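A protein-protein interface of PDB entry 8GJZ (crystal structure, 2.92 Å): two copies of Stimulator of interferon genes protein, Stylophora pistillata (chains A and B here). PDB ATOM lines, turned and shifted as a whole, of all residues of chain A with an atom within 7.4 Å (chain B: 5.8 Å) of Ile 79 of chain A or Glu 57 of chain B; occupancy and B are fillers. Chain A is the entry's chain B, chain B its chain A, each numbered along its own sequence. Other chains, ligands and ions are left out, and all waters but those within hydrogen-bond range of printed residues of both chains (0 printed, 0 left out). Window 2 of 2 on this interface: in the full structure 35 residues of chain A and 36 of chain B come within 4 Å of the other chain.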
ATOM      1  N   ASN A  75      13.340 -12.570 -32.821  1.00  0.00           N
ATOM      2  CA  ASN A  75      13.994 -11.303 -32.522  1.00  0.00           C
ATOM      3  C   ASN A  75      13.546 -10.267 -33.542  1.00  0.00           C
ATOM      4  O   ASN A  75      13.816 -10.411 -34.740  1.00  0.00           O
ATOM      5  CB  ASN A  75      15.513 -11.455 -32.546  1.00  0.00           C
ATOM      6  CG  ASN A  75      16.043 -12.190 -31.335  1.00  0.00           C
ATOM      7  OD1 ASN A  75      16.252 -11.595 -30.278  1.00  0.00           O
ATOM      8  ND2 ASN A  75      16.273 -13.489 -31.482  1.00  0.00           N
ATOM      9  N   ARG A  76      12.852  -9.232 -33.076  1.00  0.00           N
ATOM     10  CA  ARG A  76      12.347  -8.165 -33.938  1.00  0.00           C
ATOM     11  C   ARG A  76      12.947  -6.851 -33.448  1.00  0.00           C
ATOM     12  O   ARG A  76      12.340  -6.124 -32.657  1.00  0.00           O
ATOM     13  CB  ARG A  76      10.807  -8.138 -33.939  1.00  0.00           C
ATOM     14  CG  ARG A  76      10.202  -7.066 -34.831  1.00  0.00           C
ATOM     15  CD  ARG A  76      10.699  -7.183 -36.261  1.00  0.00           C
ATOM     16  NE  ARG A  76      10.247  -6.067 -37.082  1.00  0.00           N
ATOM     17  CZ  ARG A  76      10.603  -5.875 -38.345  1.00  0.00           C
ATOM     18  NH1 ARG A  76      11.418  -6.711 -38.967  1.00  0.00           N
ATOM     19  NH2 ARG A  76      10.130  -4.817 -38.998  1.00  0.00           N
ATOM     20  N   GLY A  77      14.155  -6.555 -33.920  1.00  0.00           N
ATOM     21  CA  GLY A  77      14.820  -5.311 -33.568  1.00  0.00           C
ATOM     22  C   GLY A  77      15.107  -5.157 -32.091  1.00  0.00           C
ATOM     23  O   GLY A  77      14.943  -4.062 -31.540  1.00  0.00           O
ATOM     24  N   GLY A  78      15.531  -6.231 -31.435  1.00  0.00           N
ATOM     25  CA  GLY A  78      15.825  -6.154 -30.015  1.00  0.00           C
ATOM     26  C   GLY A  78      16.562  -7.387 -29.549  1.00  0.00           C
ATOM     27  O   GLY A  78      16.627  -8.405 -30.245  1.00  0.00           O
ATOM     28  N   ILE A  79      17.123  -7.275 -28.344  1.00  0.00           N
ATOM     29  CA  ILE A  79      17.835  -8.399 -27.747  1.00  0.00           C
ATOM     30  C   ILE A  79      16.856  -9.480 -27.302  1.00  0.00           C
ATOM     31  O   ILE A  79      17.195 -10.671 -27.294  1.00  0.00           O
ATOM     32  CB  ILE A  79      18.710  -7.900 -26.582  1.00  0.00           C
ATOM     33  CG1 ILE A  79      19.476  -9.054 -25.931  1.00  0.00           C
ATOM     34  CG2 ILE A  79      17.867  -7.154 -25.560  1.00  0.00           C
ATOM     35  CD1 ILE A  79      20.524  -9.672 -26.826  1.00  0.00           C
ATOM     36  N   LYS A  80      15.633  -9.097 -26.949  1.00  0.00           N
ATOM     37  CA  LYS A  80      14.628 -10.042 -26.491  1.00  0.00           C
ATOM     38  C   LYS A  80      13.965 -10.742 -27.674  1.00  0.00           C
ATOM     39  O   LYS A  80      14.093 -10.333 -28.831  1.00  0.00           O
ATOM     40  CB  LYS A  80      13.568  -9.332 -25.653  1.00  0.00           C
ATOM     41  CG  LYS A  80      12.679  -8.410 -26.472  1.00  0.00           C
ATOM     42  CD  LYS A  80      11.676  -7.675 -25.608  1.00  0.00           C
ATOM     43  CE  LYS A  80      10.864  -6.692 -26.435  1.00  0.00           C
ATOM     44  NZ  LYS A  80       9.950  -5.870 -25.595  1.00  0.00           N
ATOM     45  N   GLU A  81      13.234 -11.812 -27.367  1.00  0.00           N
ATOM     46  CA  GLU A  81      12.463 -12.563 -28.352  1.00  0.00           C
ATOM     47  C   GLU A  81      10.986 -12.269 -28.124  1.00  0.00           C
ATOM     48  O   GLU A  81      10.422 -12.651 -27.093  1.00  0.00           O
ATOM     49  CB  GLU A  81      12.744 -14.061 -28.249  1.00  0.00           C
ATOM     50  CG  GLU A  81      14.128 -14.476 -28.718  1.00  0.00           C
ATOM     51  CD  GLU A  81      14.357 -15.972 -28.598  1.00  0.00           C
ATOM     52  OE1 GLU A  81      13.555 -16.646 -27.917  1.00  0.00           O
ATOM     53  OE2 GLU A  81      15.339 -16.473 -29.184  1.00  0.00           O
ATOM     54  N   ARG A  82      10.364 -11.594 -29.084  1.00  0.00           N
ATOM     55  CA  ARG A  82       8.944 -11.296 -28.998  1.00  0.00           C
ATOM     56  C   ARG A  82       8.119 -12.547 -29.274  1.00  0.00           C
ATOM     57  O   ARG A  82       8.518 -13.424 -30.046  1.00  0.00           O
ATOM     58  CB  ARG A  82       8.570 -10.187 -29.981  1.00  0.00           C
ATOM     59  CG  ARG A  82       9.239  -8.857 -29.670  1.00  0.00           C
ATOM     60  CD  ARG A  82       8.932  -7.814 -30.725  1.00  0.00           C
ATOM     61  NE  ARG A  82       7.498  -7.603 -30.875  1.00  0.00           N
ATOM     62  CZ  ARG A  82       6.956  -6.691 -31.669  1.00  0.00           C
ATOM     63  NH1 ARG A  82       7.702  -5.874 -32.395  1.00  0.00           N
ATOM     64  NH2 ARG A  82       5.631  -6.593 -31.736  1.00  0.00           N
ATOM     65  N   ASP B  55      22.224  -5.514 -31.208  1.00  0.00           N
ATOM     66  CA  ASP B  55      22.254  -5.561 -29.752  1.00  0.00           C
ATOM     67  C   ASP B  55      23.287  -4.578 -29.213  1.00  0.00           C
ATOM     68  O   ASP B  55      24.438  -4.564 -29.658  1.00  0.00           O
ATOM     69  CB  ASP B  55      22.570  -6.979 -29.275  1.00  0.00           C
ATOM     70  CG  ASP B  55      21.666  -8.024 -29.905  1.00  0.00           C
ATOM     71  OD1 ASP B  55      20.498  -7.702 -30.209  1.00  0.00           O
ATOM     72  OD2 ASP B  55      22.128  -9.168 -30.097  1.00  0.00           O
ATOM     73  N   ILE B  56      22.868  -3.751 -28.253  1.00  0.00           N
ATOM     74  CA  ILE B  56      23.764  -2.729 -27.725  1.00  0.00           C
ATOM     75  C   ILE B  56      24.864  -3.350 -26.875  1.00  0.00           C
ATOM     76  O   ILE B  56      25.964  -2.792 -26.773  1.00  0.00           O
ATOM     77  CB  ILE B  56      22.970  -1.673 -26.932  1.00  0.00           C
ATOM     78  CG1 ILE B  56      22.121  -2.340 -25.848  1.00  0.00           C
ATOM     79  CG2 ILE B  56      22.100  -0.845 -27.862  1.00  0.00           C
ATOM     80  CD1 ILE B  56      21.294  -1.368 -25.041  1.00  0.00           C
ATOM     81  N   GLU B  57      24.601  -4.506 -26.259  1.00  0.00           N
ATOM     82  CA  GLU B  57      25.599  -5.136 -25.402  1.00  0.00           C
ATOM     83  C   GLU B  57      26.817  -5.613 -26.179  1.00  0.00           C
ATOM     84  O   GLU B  57      27.884  -5.793 -25.582  1.00  0.00           O
ATOM     85  CB  GLU B  57      24.982  -6.315 -24.643  1.00  0.00           C
ATOM     86  CG  GLU B  57      24.600  -7.495 -25.526  1.00  0.00           C
ATOM     87  CD  GLU B  57      24.452  -8.788 -24.745  1.00  0.00           C
ATOM     88  OE1 GLU B  57      24.649  -8.767 -23.511  1.00  0.00           O
ATOM     89  OE2 GLU B  57      24.143  -9.828 -25.367  1.00  0.00           O
ATOM     90  N   GLN B  58      26.685  -5.823 -27.489  1.00  0.00           N
ATOM     91  CA  GLN B  58      27.796  -6.294 -28.305  1.00  0.00           C
ATOM     92  C   GLN B  58      28.797  -5.197 -28.635  1.00  0.00           C
ATOM     93  O   GLN B  58      29.887  -5.506 -29.131  1.00  0.00           O
ATOM     94  CB  GLN B  58      27.270  -6.906 -29.608  1.00  0.00           C
ATOM     95  CG  GLN B  58      26.155  -7.931 -29.433  1.00  0.00           C
ATOM     96  CD  GLN B  58      26.659  -9.302 -29.013  1.00  0.00           C
ATOM     97  OE1 GLN B  58      27.703  -9.428 -28.370  1.00  0.00           O
ATOM     98  NE2 GLN B  58      25.916 -10.339 -29.380  1.00  0.00           N
ATOM     99  N   ALA B  59      28.464  -3.934 -28.371  1.00  0.00           N
ATOM    100  CA  ALA B  59      29.308  -2.808 -28.749  1.00  0.00           C
ATOM    101  C   ALA B  59      29.919  -2.092 -27.552  1.00  0.00           C
ATOM    102  O   ALA B  59      30.482  -1.004 -27.716  1.00  0.00           O
ATOM    103  CB  ALA B  59      28.508  -1.818 -29.599  1.00  0.00           C
ATOM    104  N   ASP B  60      29.832  -2.670 -26.356  1.00  0.00           N
ATOM    105  CA  ASP B  60      30.345  -2.009 -25.159  1.00  0.00           C
ATOM    106  C   ASP B  60      30.544  -3.052 -24.072  1.00  0.00           C
ATOM    107  O   ASP B  60      29.598  -3.762 -23.716  1.00  0.00           O
ATOM    108  CB  ASP B  60      29.382  -0.914 -24.690  1.00  0.00           C
ATOM    109  CG  ASP B  60      30.044   0.101 -23.771  1.00  0.00           C
ATOM    110  OD1 ASP B  60      30.973  -0.273 -23.023  1.00  0.00           O
ATOM    111  OD2 ASP B  60      29.631   1.280 -23.797  1.00  0.00           O
ATOM    112  N   SER B  61      31.766  -3.140 -23.541  1.00  0.00           N
ATOM    113  CA  SER B  61      32.046  -4.050 -22.437  1.00  0.00           C
ATOM    114  C   SER B  61      31.364  -3.630 -21.142  1.00  0.00           C
ATOM    115  O   SER B  61      31.300  -4.435 -20.208  1.00  0.00           O
ATOM    116  CB  SER B  61      33.553  -4.155 -22.210  1.00  0.00           C
ATOM    117  OG  SER B  61      34.111  -2.886 -21.916  1.00  0.00           O
ATOM    118  N   VAL B  63      28.149  -2.731 -21.059  1.00  0.00           N
ATOM    119  CA  VAL B  63      26.739  -3.062 -21.233  1.00  0.00           C
ATOM    120  C   VAL B  63      26.606  -4.576 -21.325  1.00  0.00           C
ATOM    121  O   VAL B  63      27.291  -5.218 -22.130  1.00  0.00           O
ATOM    122  CB  VAL B  63      26.154  -2.386 -22.484  1.00  0.00           C
ATOM    123  CG1 VAL B  63      24.659  -2.635 -22.570  1.00  0.00           C
ATOM    124  CG2 VAL B  63      26.459  -0.897 -22.477  1.00  0.00           C
ATOM    125  N   LYS B  64      25.720  -5.141 -20.508  1.00  0.00           N
ATOM    126  CA  LYS B  64      25.505  -6.581 -20.474  1.00  0.00           C
ATOM    127  C   LYS B  64      24.033  -6.870 -20.239  1.00  0.00           C
ATOM    128  O   LYS B  64      23.442  -6.362 -19.281  1.00  0.00           O
ATOM    129  CB  LYS B  64      26.354  -7.245 -19.382  1.00  0.00           C
ATOM    130  CG  LYS B  64      25.934  -8.671 -19.052  1.00  0.00           C
ATOM    131  CD  LYS B  64      26.782  -9.263 -17.933  1.00  0.00           C
ATOM    132  CE  LYS B  64      26.139 -10.519 -17.353  1.00  0.00           C
ATOM    133  NZ  LYS B  64      25.899 -11.569 -18.381  1.00  0.00           N
ATOM    134  N   TRP B  65      23.447  -7.679 -21.118  1.00  0.00           N
ATOM    135  CA  TRP B  65      22.088  -8.164 -20.920  1.00  0.00           C
ATOM    136  C   TRP B  65      22.058  -9.139 -19.748  1.00  0.00           C
ATOM    137  O   TRP B  65      22.870 -10.069 -19.683  1.00  0.00           O
ATOM    138  CB  TRP B  65      21.592  -8.839 -22.197  1.00  0.00           C
ATOM    139  CG  TRP B  65      20.203  -9.380 -22.124  1.00  0.00           C
ATOM    140  CD1 TRP B  65      19.139  -8.833 -21.467  1.00  0.00           C
ATOM    141  CD2 TRP B  65      19.723 -10.583 -22.733  1.00  0.00           C
ATOM    142  NE1 TRP B  65      18.024  -9.622 -21.634  1.00  0.00           N
ATOM    143  CE2 TRP B  65      18.358 -10.704 -22.406  1.00  0.00           C
ATOM    144  CE3 TRP B  65      20.316 -11.571 -23.526  1.00  0.00           C
ATOM    145  CZ2 TRP B  65      17.579 -11.771 -22.842  1.00  0.00           C
ATOM    146  CZ3 TRP B  65      19.540 -12.629 -23.956  1.00  0.00           C
ATOM    147  CH2 TRP B  65      18.189 -12.721 -23.614  1.00  0.00           C
ATOM    148  N   ASN B  68      15.242 -10.725 -18.604  1.00  0.00           N
ATOM    149  CA  ASN B  68      14.025 -10.002 -18.924  1.00  0.00           C
ATOM    150  C   ASN B  68      13.159  -9.844 -17.682  1.00  0.00           C
ATOM    151  O   ASN B  68      13.270 -10.604 -16.716  1.00  0.00           O
ATOM    152  CB  ASN B  68      13.224 -10.718 -20.020  1.00  0.00           C
ATOM    153  CG  ASN B  68      13.997 -10.854 -21.316  1.00  0.00           C
ATOM    154  OD1 ASN B  68      14.814  -9.999 -21.659  1.00  0.00           O
ATOM    155  ND2 ASN B  68      13.741 -11.931 -22.045  1.00  0.00           N
ATOM    156  N   ALA B  87      13.520  -6.263 -21.650  1.00  0.00           N
ATOM    157  CA  ALA B  87      14.860  -6.741 -21.347  1.00  0.00           C
ATOM    158  C   ALA B  87      15.581  -5.732 -20.466  1.00  0.00           C
ATOM    159  O   ALA B  87      15.465  -4.520 -20.667  1.00  0.00           O
ATOM    160  CB  ALA B  87      15.655  -6.979 -22.632  1.00  0.00           C
ATOM    161  N   HIS B  89      19.182  -4.303 -19.032  1.00  0.00           N
ATOM    162  CA  HIS B  89      20.602  -4.209 -19.334  1.00  0.00           C
ATOM    163  C   HIS B  89      21.352  -3.653 -18.132  1.00  0.00           C
ATOM    164  O   HIS B  89      20.910  -2.686 -17.503  1.00  0.00           O
ATOM    165  CB  HIS B  89      20.851  -3.333 -20.565  1.00  0.00           C
ATOM    166  CG  HIS B  89      20.489  -3.996 -21.858  1.00  0.00           C
ATOM    167  ND1 HIS B  89      21.405  -4.689 -22.620  1.00  0.00           N
ATOM    168  CD2 HIS B  89      19.312  -4.076 -22.521  1.00  0.00           C
ATOM    169  CE1 HIS B  89      20.809  -5.165 -23.698  1.00  0.00           C
ATOM    170  NE2 HIS B  89      19.538  -4.808 -23.663  1.00  0.00           N
ATOM    171  N   VAL B 107      16.115  -0.527 -21.902  1.00  0.00           N
ATOM    172  CA  VAL B 107      16.464   0.137 -23.153  1.00  0.00           C
ATOM    173  C   VAL B 107      15.919  -0.688 -24.310  1.00  0.00           C
ATOM    174  O   VAL B 107      16.142  -1.902 -24.370  1.00  0.00           O
ATOM    175  CB  VAL B 107      17.986   0.325 -23.293  1.00  0.00           C
ATOM    176  CG1 VAL B 107      18.300   1.257 -24.452  1.00  0.00           C
ATOM    177  CG2 VAL B 107      18.575   0.851 -22.000  1.00  0.00           C
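Printed residues of chain A that touch a printed residue of chain B: Gly 78 and Ile 79.
Of the 14 printed residues of chain B, 5 touch a printed residue of chain A.
Printed residues of chain B that touch a printed residue of chain A: Asp 55, Glu 57, Trp 65, Ala 87 and His 89.
Among the printed residues, no Asp or Glu carboxylate lies within 4 Å of a Lys or Arg side-chain nitrogen of the other chain.
Gly 78 of chain A touches Asp 55 of chain B.
CD1 of Ile 79 of chain A touches CG of Asp 55 of chain B, 3.7 Å away.
Glu 57 of chain B touches Ile 79 of chain A.
CG1 of Ile 79 of chain A touches CD2 of Trp 65 of chain B, 3.6 Å away.
Ile 79 of chain A touches Ala 87 of chain B (CG2 to CB, 3.7 Å).
CG2 of Ile 79 of chain A touches NE2 of His 89 of chain B (3.4 Å).
No position is printed for both chains.
Of the 6 pairs that touch across the chains among the printed residues, none has its exchanged pair printed and touching as well.
The side-chain carboxylate (OE1) of Glu 57 of chain B lies within hydrogen-bond range of the backbone NH (N) of Trp 65 of chain B, at 2.9 Å.
The indole nitrogen (NE1) of Trp 65 of chain B is in hydrogen-bond range of the side-chain amide oxygen (OD1) of Asn 68 of chain B, 3.2 Å away.
The backbone carbonyl oxygen of Gly 78 of chain A lies close to the side-chain amide oxygen of Asn 75 of chain A (3.2 Å).
The side-chain amide oxygen of Asn 75 of chain A lies close to the backbone carbonyl oxygen of Ile 79 of chain A, at 3.3 Å.
Ile 79 of chain A touches just these residues of chain B: Asp 55 (3.7 Å), Glu 57 (3.9 Å), Trp 65 (3.6 Å), Ala 87 (3.7 Å) and His 89 (3.4 Å).
Glu 57 of chain B touches one residue of chain A.
Of the printed residues of chain A, Ala 87 of chain B touches Ile 79 (3.7 Å).
Printed residues of chain B within 4 Å of Gly 78 of chain A: Asp 55.
The nearest residue of chain B that does not touch Ile 79 of chain A is Val 107 of chain B (5.7 Å).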
